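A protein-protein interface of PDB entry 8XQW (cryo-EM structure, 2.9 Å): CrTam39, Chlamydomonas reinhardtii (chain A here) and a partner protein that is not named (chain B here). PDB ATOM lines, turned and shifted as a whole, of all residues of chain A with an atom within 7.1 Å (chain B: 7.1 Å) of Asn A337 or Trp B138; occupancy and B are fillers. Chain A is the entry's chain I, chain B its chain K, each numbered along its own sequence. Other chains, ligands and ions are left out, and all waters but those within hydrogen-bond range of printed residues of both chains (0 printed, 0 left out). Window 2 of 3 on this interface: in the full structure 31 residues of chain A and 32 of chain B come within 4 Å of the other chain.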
ATOM      1  N   VAL A 332      22.942   8.703 -36.782  1.00  0.00           N
ATOM      2  CA  VAL A 332      22.190   7.953 -35.790  1.00  0.00           C
ATOM      3  C   VAL A 332      23.150   6.972 -35.148  1.00  0.00           C
ATOM      4  O   VAL A 332      23.571   6.000 -35.780  1.00  0.00           O
ATOM      5  CB  VAL A 332      20.997   7.229 -36.412  1.00  0.00           C
ATOM      6  CG1 VAL A 332      20.185   6.573 -35.335  1.00  0.00           C
ATOM      7  CG2 VAL A 332      20.158   8.204 -37.190  1.00  0.00           C
ATOM      8  N   ALA A 333      23.502   7.215 -33.895  1.00  0.00           N
ATOM      9  CA  ALA A 333      24.467   6.386 -33.208  1.00  0.00           C
ATOM     10  C   ALA A 333      24.174   6.467 -31.720  1.00  0.00           C
ATOM     11  O   ALA A 333      23.158   7.023 -31.304  1.00  0.00           O
ATOM     12  CB  ALA A 333      25.887   6.830 -33.557  1.00  0.00           C
ATOM     13  N   LEU A 334      25.037   5.921 -30.934  1.00  0.00           N
ATOM     14  CA  LEU A 334      24.836   6.118 -29.518  1.00  0.00           C
ATOM     15  C   LEU A 334      25.332   7.505 -29.124  1.00  0.00           C
ATOM     16  O   LEU A 334      26.285   8.016 -29.708  1.00  0.00           O
ATOM     17  CB  LEU A 334      25.563   5.044 -28.731  1.00  0.00           C
ATOM     18  CG  LEU A 334      25.283   3.606 -29.142  1.00  0.00           C
ATOM     19  CD1 LEU A 334      26.350   2.710 -28.653  1.00  0.00           C
ATOM     20  CD2 LEU A 334      23.992   3.160 -28.575  1.00  0.00           C
ATOM     21  N   PRO A 335      24.686   8.150 -28.155  1.00  0.00           N
ATOM     22  CA  PRO A 335      24.970   9.555 -27.904  1.00  0.00           C
ATOM     23  C   PRO A 335      26.379   9.742 -27.377  1.00  0.00           C
ATOM     24  O   PRO A 335      26.999   8.792 -26.870  1.00  0.00           O
ATOM     25  CB  PRO A 335      23.922   9.941 -26.858  1.00  0.00           C
ATOM     26  CG  PRO A 335      23.522   8.684 -26.266  1.00  0.00           C
ATOM     27  CD  PRO A 335      23.569   7.678 -27.331  1.00  0.00           C
ATOM     28  N   PRO A 336      26.921  10.949 -27.476  1.00  0.00           N
ATOM     29  CA  PRO A 336      28.308  11.172 -27.060  1.00  0.00           C
ATOM     30  C   PRO A 336      28.507  11.011 -25.566  1.00  0.00           C
ATOM     31  O   PRO A 336      27.616  11.290 -24.767  1.00  0.00           O
ATOM     32  CB  PRO A 336      28.569  12.612 -27.497  1.00  0.00           C
ATOM     33  CG  PRO A 336      27.635  12.827 -28.586  1.00  0.00           C
ATOM     34  CD  PRO A 336      26.403  12.092 -28.232  1.00  0.00           C
ATOM     35  N   ASN A 337      29.698  10.565 -25.202  1.00  0.00           N
ATOM     36  CA  ASN A 337      30.098  10.339 -23.828  1.00  0.00           C
ATOM     37  C   ASN A 337      30.613  11.611 -23.202  1.00  0.00           C
ATOM     38  O   ASN A 337      30.850  12.597 -23.882  1.00  0.00           O
ATOM     39  CB  ASN A 337      31.227   9.330 -23.773  1.00  0.00           C
ATOM     40  CG  ASN A 337      30.758   7.960 -23.858  1.00  0.00           C
ATOM     41  OD1 ASN A 337      31.522   7.056 -24.131  1.00  0.00           O
ATOM     42  ND2 ASN A 337      29.492   7.768 -23.616  1.00  0.00           N
ATOM     43  N   PRO A 338      30.825  11.608 -21.891  1.00  0.00           N
ATOM     44  CA  PRO A 338      31.748  12.572 -21.303  1.00  0.00           C
ATOM     45  C   PRO A 338      33.187  12.313 -21.660  1.00  0.00           C
ATOM     46  O   PRO A 338      34.057  13.063 -21.215  1.00  0.00           O
ATOM     47  CB  PRO A 338      31.527  12.392 -19.809  1.00  0.00           C
ATOM     48  CG  PRO A 338      30.216  11.863 -19.697  1.00  0.00           C
ATOM     49  CD  PRO A 338      29.975  11.006 -20.866  1.00  0.00           C
ATOM     50  N   GLY A 339      33.474  11.281 -22.429  1.00  0.00           N
ATOM     51  CA  GLY A 339      34.837  10.968 -22.770  1.00  0.00           C
ATOM     52  C   GLY A 339      35.184  11.575 -24.100  1.00  0.00           C
ATOM     53  O   GLY A 339      36.346  11.852 -24.378  1.00  0.00           O
ATOM     54  N   ALA A 340      34.179  11.793 -24.931  1.00  0.00           N
ATOM     55  CA  ALA A 340      34.392  12.430 -26.214  1.00  0.00           C
ATOM     56  C   ALA A 340      34.548  13.934 -26.106  1.00  0.00           C
ATOM     57  O   ALA A 340      35.249  14.528 -26.926  1.00  0.00           O
ATOM     58  CB  ALA A 340      33.233  12.120 -27.149  1.00  0.00           C
ATOM     59  N   VAL A 341      33.928  14.562 -25.113  1.00  0.00           N
ATOM     60  CA  VAL A 341      33.951  16.005 -24.955  1.00  0.00           C
ATOM     61  C   VAL A 341      34.959  16.451 -23.916  1.00  0.00           C
ATOM     62  O   VAL A 341      34.905  17.593 -23.473  1.00  0.00           O
ATOM     63  CB  VAL A 341      32.561  16.550 -24.612  1.00  0.00           C
ATOM     64  CG1 VAL A 341      31.591  16.206 -25.677  1.00  0.00           C
ATOM     65  CG2 VAL A 341      32.107  16.006 -23.303  1.00  0.00           C
ATOM     66  N   PHE A 342      35.878  15.588 -23.500  1.00  0.00           N
ATOM     67  CA  PHE A 342      36.876  16.036 -22.539  1.00  0.00           C
ATOM     68  C   PHE A 342      37.763  17.106 -23.142  1.00  0.00           C
ATOM     69  O   PHE A 342      38.101  18.088 -22.479  1.00  0.00           O
ATOM     70  CB  PHE A 342      37.721  14.870 -22.048  1.00  0.00           C
ATOM     71  CG  PHE A 342      38.860  15.280 -21.163  1.00  0.00           C
ATOM     72  CD1 PHE A 342      38.631  15.836 -19.932  1.00  0.00           C
ATOM     73  CD2 PHE A 342      40.160  15.110 -21.561  1.00  0.00           C
ATOM     74  CE1 PHE A 342      39.669  16.208 -19.133  1.00  0.00           C
ATOM     75  CE2 PHE A 342      41.191  15.479 -20.752  1.00  0.00           C
ATOM     76  CZ  PHE A 342      40.946  16.033 -19.549  1.00  0.00           C
ATOM     77  N   VAL A 353      26.492  17.810 -22.201  1.00  0.00           N
ATOM     78  CA  VAL A 353      26.705  16.364 -22.196  1.00  0.00           C
ATOM     79  C   VAL A 353      26.867  15.848 -20.771  1.00  0.00           C
ATOM     80  O   VAL A 353      26.267  14.837 -20.386  1.00  0.00           O
ATOM     81  CB  VAL A 353      27.913  15.998 -23.068  1.00  0.00           C
ATOM     82  CG1 VAL A 353      28.360  14.627 -22.763  1.00  0.00           C
ATOM     83  CG2 VAL A 353      27.536  16.077 -24.496  1.00  0.00           C
ATOM     84  N   TRP A 354      27.682  16.529 -19.968  1.00  0.00           N
ATOM     85  CA  TRP A 354      27.831  16.137 -18.574  1.00  0.00           C
ATOM     86  C   TRP A 354      26.491  16.118 -17.868  1.00  0.00           C
ATOM     87  O   TRP A 354      26.212  15.220 -17.076  1.00  0.00           O
ATOM     88  CB  TRP A 354      28.767  17.087 -17.853  1.00  0.00           C
ATOM     89  CG  TRP A 354      30.172  16.938 -18.179  1.00  0.00           C
ATOM     90  CD1 TRP A 354      30.703  16.273 -19.221  1.00  0.00           C
ATOM     91  CD2 TRP A 354      31.256  17.498 -17.459  1.00  0.00           C
ATOM     92  NE1 TRP A 354      32.065  16.373 -19.200  1.00  0.00           N
ATOM     93  CE2 TRP A 354      32.428  17.120 -18.116  1.00  0.00           C
ATOM     94  CE3 TRP A 354      31.352  18.271 -16.309  1.00  0.00           C
ATOM     95  CZ2 TRP A 354      33.680  17.501 -17.670  1.00  0.00           C
ATOM     96  CZ3 TRP A 354      32.590  18.642 -15.871  1.00  0.00           C
ATOM     97  CH2 TRP A 354      33.735  18.258 -16.542  1.00  0.00           C
ATOM     98  N   TRP A 357      24.471  12.975 -18.791  1.00  0.00           N
ATOM     99  CA  TRP A 357      24.976  11.702 -18.300  1.00  0.00           C
ATOM    100  C   TRP A 357      24.979  11.594 -16.785  1.00  0.00           C
ATOM    101  O   TRP A 357      25.332  10.541 -16.263  1.00  0.00           O
ATOM    102  CB  TRP A 357      26.377  11.449 -18.844  1.00  0.00           C
ATOM    103  CG  TRP A 357      26.337  10.886 -20.199  1.00  0.00           C
ATOM    104  CD1 TRP A 357      26.367  11.570 -21.362  1.00  0.00           C
ATOM    105  CD2 TRP A 357      26.219   9.516 -20.543  1.00  0.00           C
ATOM    106  NE1 TRP A 357      26.287  10.713 -22.414  1.00  0.00           N
ATOM    107  CE2 TRP A 357      26.196   9.438 -21.934  1.00  0.00           C
ATOM    108  CE3 TRP A 357      26.135   8.341 -19.808  1.00  0.00           C
ATOM    109  CZ2 TRP A 357      26.094   8.241 -22.603  1.00  0.00           C
ATOM    110  CZ3 TRP A 357      26.039   7.160 -20.474  1.00  0.00           C
ATOM    111  CH2 TRP A 357      26.017   7.115 -21.855  1.00  0.00           C
ATOM    112  N   ALA B 134      32.550  10.267 -39.428  1.00  0.00           N
ATOM    113  CA  ALA B 134      31.992   8.946 -39.644  1.00  0.00           C
ATOM    114  C   ALA B 134      32.910   7.863 -39.129  1.00  0.00           C
ATOM    115  O   ALA B 134      32.472   6.724 -38.959  1.00  0.00           O
ATOM    116  CB  ALA B 134      31.716   8.724 -41.126  1.00  0.00           C
ATOM    117  N   GLU B 135      34.164   8.201 -38.874  1.00  0.00           N
ATOM    118  CA  GLU B 135      35.091   7.357 -38.154  1.00  0.00           C
ATOM    119  C   GLU B 135      35.041   7.601 -36.662  1.00  0.00           C
ATOM    120  O   GLU B 135      35.829   7.019 -35.919  1.00  0.00           O
ATOM    121  CB  GLU B 135      36.499   7.586 -38.677  1.00  0.00           C
ATOM    122  CG  GLU B 135      36.608   7.433 -40.157  1.00  0.00           C
ATOM    123  CD  GLU B 135      38.025   7.176 -40.593  1.00  0.00           C
ATOM    124  OE1 GLU B 135      38.948   7.484 -39.816  1.00  0.00           O
ATOM    125  OE2 GLU B 135      38.230   6.658 -41.707  1.00  0.00           O
ATOM    126  N   LYS B 136      34.129   8.451 -36.208  1.00  0.00           N
ATOM    127  CA  LYS B 136      33.931   8.691 -34.789  1.00  0.00           C
ATOM    128  C   LYS B 136      32.526   8.341 -34.333  1.00  0.00           C
ATOM    129  O   LYS B 136      32.078   8.860 -33.313  1.00  0.00           O
ATOM    130  CB  LYS B 136      34.219  10.146 -34.452  1.00  0.00           C
ATOM    131  CG  LYS B 136      35.576  10.597 -34.859  1.00  0.00           C
ATOM    132  CD  LYS B 136      35.676  12.068 -34.715  1.00  0.00           C
ATOM    133  CE  LYS B 136      37.013  12.463 -34.205  1.00  0.00           C
ATOM    134  NZ  LYS B 136      37.003  13.878 -33.786  1.00  0.00           N
ATOM    135  N   ARG B 137      31.813   7.498 -35.062  1.00  0.00           N
ATOM    136  CA  ARG B 137      30.500   7.072 -34.622  1.00  0.00           C
ATOM    137  C   ARG B 137      30.640   5.998 -33.565  1.00  0.00           C
ATOM    138  O   ARG B 137      31.415   5.059 -33.729  1.00  0.00           O
ATOM    139  CB  ARG B 137      29.700   6.530 -35.789  1.00  0.00           C
ATOM    140  CG  ARG B 137      29.149   7.555 -36.693  1.00  0.00           C
ATOM    141  CD  ARG B 137      28.511   6.895 -37.865  1.00  0.00           C
ATOM    142  NE  ARG B 137      27.228   6.322 -37.510  1.00  0.00           N
ATOM    143  CZ  ARG B 137      26.948   5.033 -37.604  1.00  0.00           C
ATOM    144  NH1 ARG B 137      25.758   4.593 -37.259  1.00  0.00           N
ATOM    145  NH2 ARG B 137      27.858   4.193 -38.038  1.00  0.00           N
ATOM    146  N   TRP B 138      29.885   6.124 -32.485  1.00  0.00           N
ATOM    147  CA  TRP B 138      29.860   5.114 -31.441  1.00  0.00           C
ATOM    148  C   TRP B 138      28.717   4.166 -31.751  1.00  0.00           C
ATOM    149  O   TRP B 138      27.555   4.566 -31.747  1.00  0.00           O
ATOM    150  CB  TRP B 138      29.708   5.767 -30.075  1.00  0.00           C
ATOM    151  CG  TRP B 138      29.801   4.843 -28.913  1.00  0.00           C
ATOM    152  CD1 TRP B 138      30.429   3.648 -28.860  1.00  0.00           C
ATOM    153  CD2 TRP B 138      29.243   5.054 -27.625  1.00  0.00           C
ATOM    154  NE1 TRP B 138      30.291   3.092 -27.624  1.00  0.00           N
ATOM    155  CE2 TRP B 138      29.559   3.944 -26.847  1.00  0.00           C
ATOM    156  CE3 TRP B 138      28.493   6.076 -27.058  1.00  0.00           C
ATOM    157  CZ2 TRP B 138      29.166   3.834 -25.533  1.00  0.00           C
ATOM    158  CZ3 TRP B 138      28.104   5.961 -25.763  1.00  0.00           C
ATOM    159  CH2 TRP B 138      28.434   4.854 -25.014  1.00  0.00           C
ATOM    160  N   THR B 139      29.046   2.920 -32.063  1.00  0.00           N
ATOM    161  CA  THR B 139      28.076   1.896 -32.399  1.00  0.00           C
ATOM    162  C   THR B 139      28.448   0.629 -31.655  1.00  0.00           C
ATOM    163  O   THR B 139      29.534   0.522 -31.104  1.00  0.00           O
ATOM    164  CB  THR B 139      28.039   1.630 -33.899  1.00  0.00           C
ATOM    165  OG1 THR B 139      29.353   1.347 -34.364  1.00  0.00           O
ATOM    166  CG2 THR B 139      27.537   2.829 -34.621  1.00  0.00           C
ATOM    167  N   LEU B 140      27.548  -0.350 -31.657  1.00  0.00           N
ATOM    168  CA  LEU B 140      27.800  -1.568 -30.900  1.00  0.00           C
ATOM    169  C   LEU B 140      28.913  -2.403 -31.505  1.00  0.00           C
ATOM    170  O   LEU B 140      29.549  -3.173 -30.790  1.00  0.00           O
ATOM    171  CB  LEU B 140      26.542  -2.413 -30.798  1.00  0.00           C
ATOM    172  CG  LEU B 140      25.401  -1.844 -29.969  1.00  0.00           C
ATOM    173  CD1 LEU B 140      24.121  -2.544 -30.297  1.00  0.00           C
ATOM    174  CD2 LEU B 140      25.698  -2.001 -28.515  1.00  0.00           C
ATOM    175  N   PHE B 141      29.153  -2.300 -32.805  1.00  0.00           N
ATOM    176  CA  PHE B 141      30.270  -3.035 -33.374  1.00  0.00           C
ATOM    177  C   PHE B 141      31.592  -2.442 -32.934  1.00  0.00           C
ATOM    178  O   PHE B 141      32.562  -3.167 -32.719  1.00  0.00           O
ATOM    179  CB  PHE B 141      30.192  -3.049 -34.891  1.00  0.00           C
ATOM    180  CG  PHE B 141      31.471  -3.465 -35.554  1.00  0.00           C
ATOM    181  CD1 PHE B 141      31.812  -4.791 -35.650  1.00  0.00           C
ATOM    182  CD2 PHE B 141      32.333  -2.531 -36.082  1.00  0.00           C
ATOM    183  CE1 PHE B 141      32.984  -5.173 -36.249  1.00  0.00           C
ATOM    184  CE2 PHE B 141      33.508  -2.921 -36.675  1.00  0.00           C
ATOM    185  CZ  PHE B 141      33.823  -4.239 -36.762  1.00  0.00           C
ATOM    186  N   SER B 142      31.659  -1.126 -32.799  1.00  0.00           N
ATOM    187  CA  SER B 142      32.922  -0.483 -32.496  1.00  0.00           C
ATOM    188  C   SER B 142      33.344  -0.640 -31.051  1.00  0.00           C
ATOM    189  O   SER B 142      34.544  -0.611 -30.772  1.00  0.00           O
ATOM    190  CB  SER B 142      32.849   0.990 -32.831  1.00  0.00           C
ATOM    191  OG  SER B 142      32.212   1.677 -31.792  1.00  0.00           O
ATOM    192  N   THR B 143      32.416  -0.828 -30.122  1.00  0.00           N
ATOM    193  CA  THR B 143      32.856  -1.031 -28.753  1.00  0.00           C
ATOM    194  C   THR B 143      33.387  -2.433 -28.501  1.00  0.00           C
ATOM    195  O   THR B 143      33.836  -2.705 -27.391  1.00  0.00           O
ATOM    196  CB  THR B 143      31.744  -0.718 -27.756  1.00  0.00           C
ATOM    197  OG1 THR B 143      31.445  -1.883 -27.005  1.00  0.00           O
ATOM    198  CG2 THR B 143      30.519  -0.294 -28.424  1.00  0.00           C
ATOM    199  N   PHE B 252      23.076   1.470 -37.933  1.00  0.00           N
ATOM    200  CA  PHE B 252      22.357   2.242 -36.929  1.00  0.00           C
ATOM    201  C   PHE B 252      23.221   2.221 -35.689  1.00  0.00           C
ATOM    202  O   PHE B 252      24.442   2.207 -35.803  1.00  0.00           O
ATOM    203  CB  PHE B 252      20.948   1.711 -36.691  1.00  0.00           C
ATOM    204  CG  PHE B 252      19.936   2.265 -37.651  1.00  0.00           C
ATOM    205  CD1 PHE B 252      19.831   3.623 -37.857  1.00  0.00           C
ATOM    206  CD2 PHE B 252      19.128   1.430 -38.383  1.00  0.00           C
ATOM    207  CE1 PHE B 252      18.928   4.124 -38.752  1.00  0.00           C
ATOM    208  CE2 PHE B 252      18.227   1.934 -39.276  1.00  0.00           C
ATOM    209  CZ  PHE B 252      18.128   3.276 -39.460  1.00  0.00           C
ATOM    210  N   TRP B 253      22.629   2.293 -34.508  1.00  0.00           N
ATOM    211  CA  TRP B 253      23.385   1.934 -33.315  1.00  0.00           C
ATOM    212  C   TRP B 253      24.092   0.593 -33.452  1.00  0.00           C
ATOM    213  O   TRP B 253      24.975   0.287 -32.657  1.00  0.00           O
ATOM    214  CB  TRP B 253      22.476   1.875 -32.092  1.00  0.00           C
ATOM    215  CG  TRP B 253      21.380   2.843 -32.134  1.00  0.00           C
ATOM    216  CD1 TRP B 253      21.418   4.128 -31.715  1.00  0.00           C
ATOM    217  CD2 TRP B 253      20.065   2.614 -32.622  1.00  0.00           C
ATOM    218  NE1 TRP B 253      20.208   4.725 -31.917  1.00  0.00           N
ATOM    219  CE2 TRP B 253      19.355   3.814 -32.477  1.00  0.00           C
ATOM    220  CE3 TRP B 253      19.416   1.509 -33.173  1.00  0.00           C
ATOM    221  CZ2 TRP B 253      18.030   3.943 -32.862  1.00  0.00           C
ATOM    222  CZ3 TRP B 253      18.106   1.640 -33.555  1.00  0.00           C
ATOM    223  CH2 TRP B 253      17.425   2.847 -33.397  1.00  0.00           C
ATOM    224  N   LEU B 254      23.727  -0.221 -34.439  1.00  0.00           N
ATOM    225  CA  LEU B 254      24.283  -1.566 -34.533  1.00  0.00           C
ATOM    226  C   LEU B 254      25.715  -1.556 -35.039  1.00  0.00           C
ATOM    227  O   LEU B 254      26.628  -1.979 -34.336  1.00  0.00           O
ATOM    228  CB  LEU B 254      23.414  -2.438 -35.432  1.00  0.00           C
ATOM    229  CG  LEU B 254      24.002  -3.824 -35.665  1.00  0.00           C
ATOM    230  CD1 LEU B 254      24.090  -4.556 -34.359  1.00  0.00           C
ATOM    231  CD2 LEU B 254      23.172  -4.611 -36.639  1.00  0.00           C
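Printed residues of chain B within 4 Å of Val A332: Arg B137 (3.0 Å), Phe B252 (3.8 Å) and Trp B253 (3.9 Å). Of the printed residues of chain B, Ala A333 touches Trp B138 and Trp B253. Printed residues of chain B within 4 Å of Pro A335: Trp B138 (3.1 Å). Asn A337 touches one residue of chain B. Gly A339 touches none of the printed residues of chain B. Glu B135 touches none of the printed residues of chain A. Trp B138 touches just these residues of chain A: Ala A333 (3.3 Å), Leu A334 (3.0 Å), Pro A335 (3.1 Å) and Asn A337 (3.1 Å).
NH1 of Arg B137 sits at hydrogen-bond distance from O of Phe B252, at 3.1 Å. The backbone NH of Leu B140 sits at hydrogen-bond distance from the backbone carbonyl oxygen of Trp B253, at 2.8 Å.
Among the printed residues, merely in contact across the chains: Val A332 with Phe B252 (3.8 Å), Val A332 with Trp B253 (3.9 Å), Ala A333 with Trp B138 (3.3 Å), Ala A333 with Trp B253 (3.4 Å), Pro A335 with Trp B138 (3.1 Å) and Asn A337 with Trp B138 (3.1 Å).
Printed residues of chain A that touch a printed residue of chain B: Val A332, Ala A333, Leu A334, Pro A335 and Asn A337. Hydrophobic or aromatic side chains of chain A within 4 Å of the printed part of chain B: Val A332, Ala A333 and Leu A334. Along chain A the printed residues that touch a printed residue of chain B span positions 332 to 337. Among the printed residues, no Asp or Glu carboxylate lies within 4 Å of a Lys or Arg side-chain nitrogen of the other chain.
The guanidinium group (NH1) of Arg B137 sits at hydrogen-bond distance from the backbone carbonyl oxygen (O) of Val A332 (3.0 Å). The backbone carbonyl oxygen (O) of Trp B138 is in hydrogen-bond range of the backbone NH (N) of Leu A334, 3.0 Å away.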
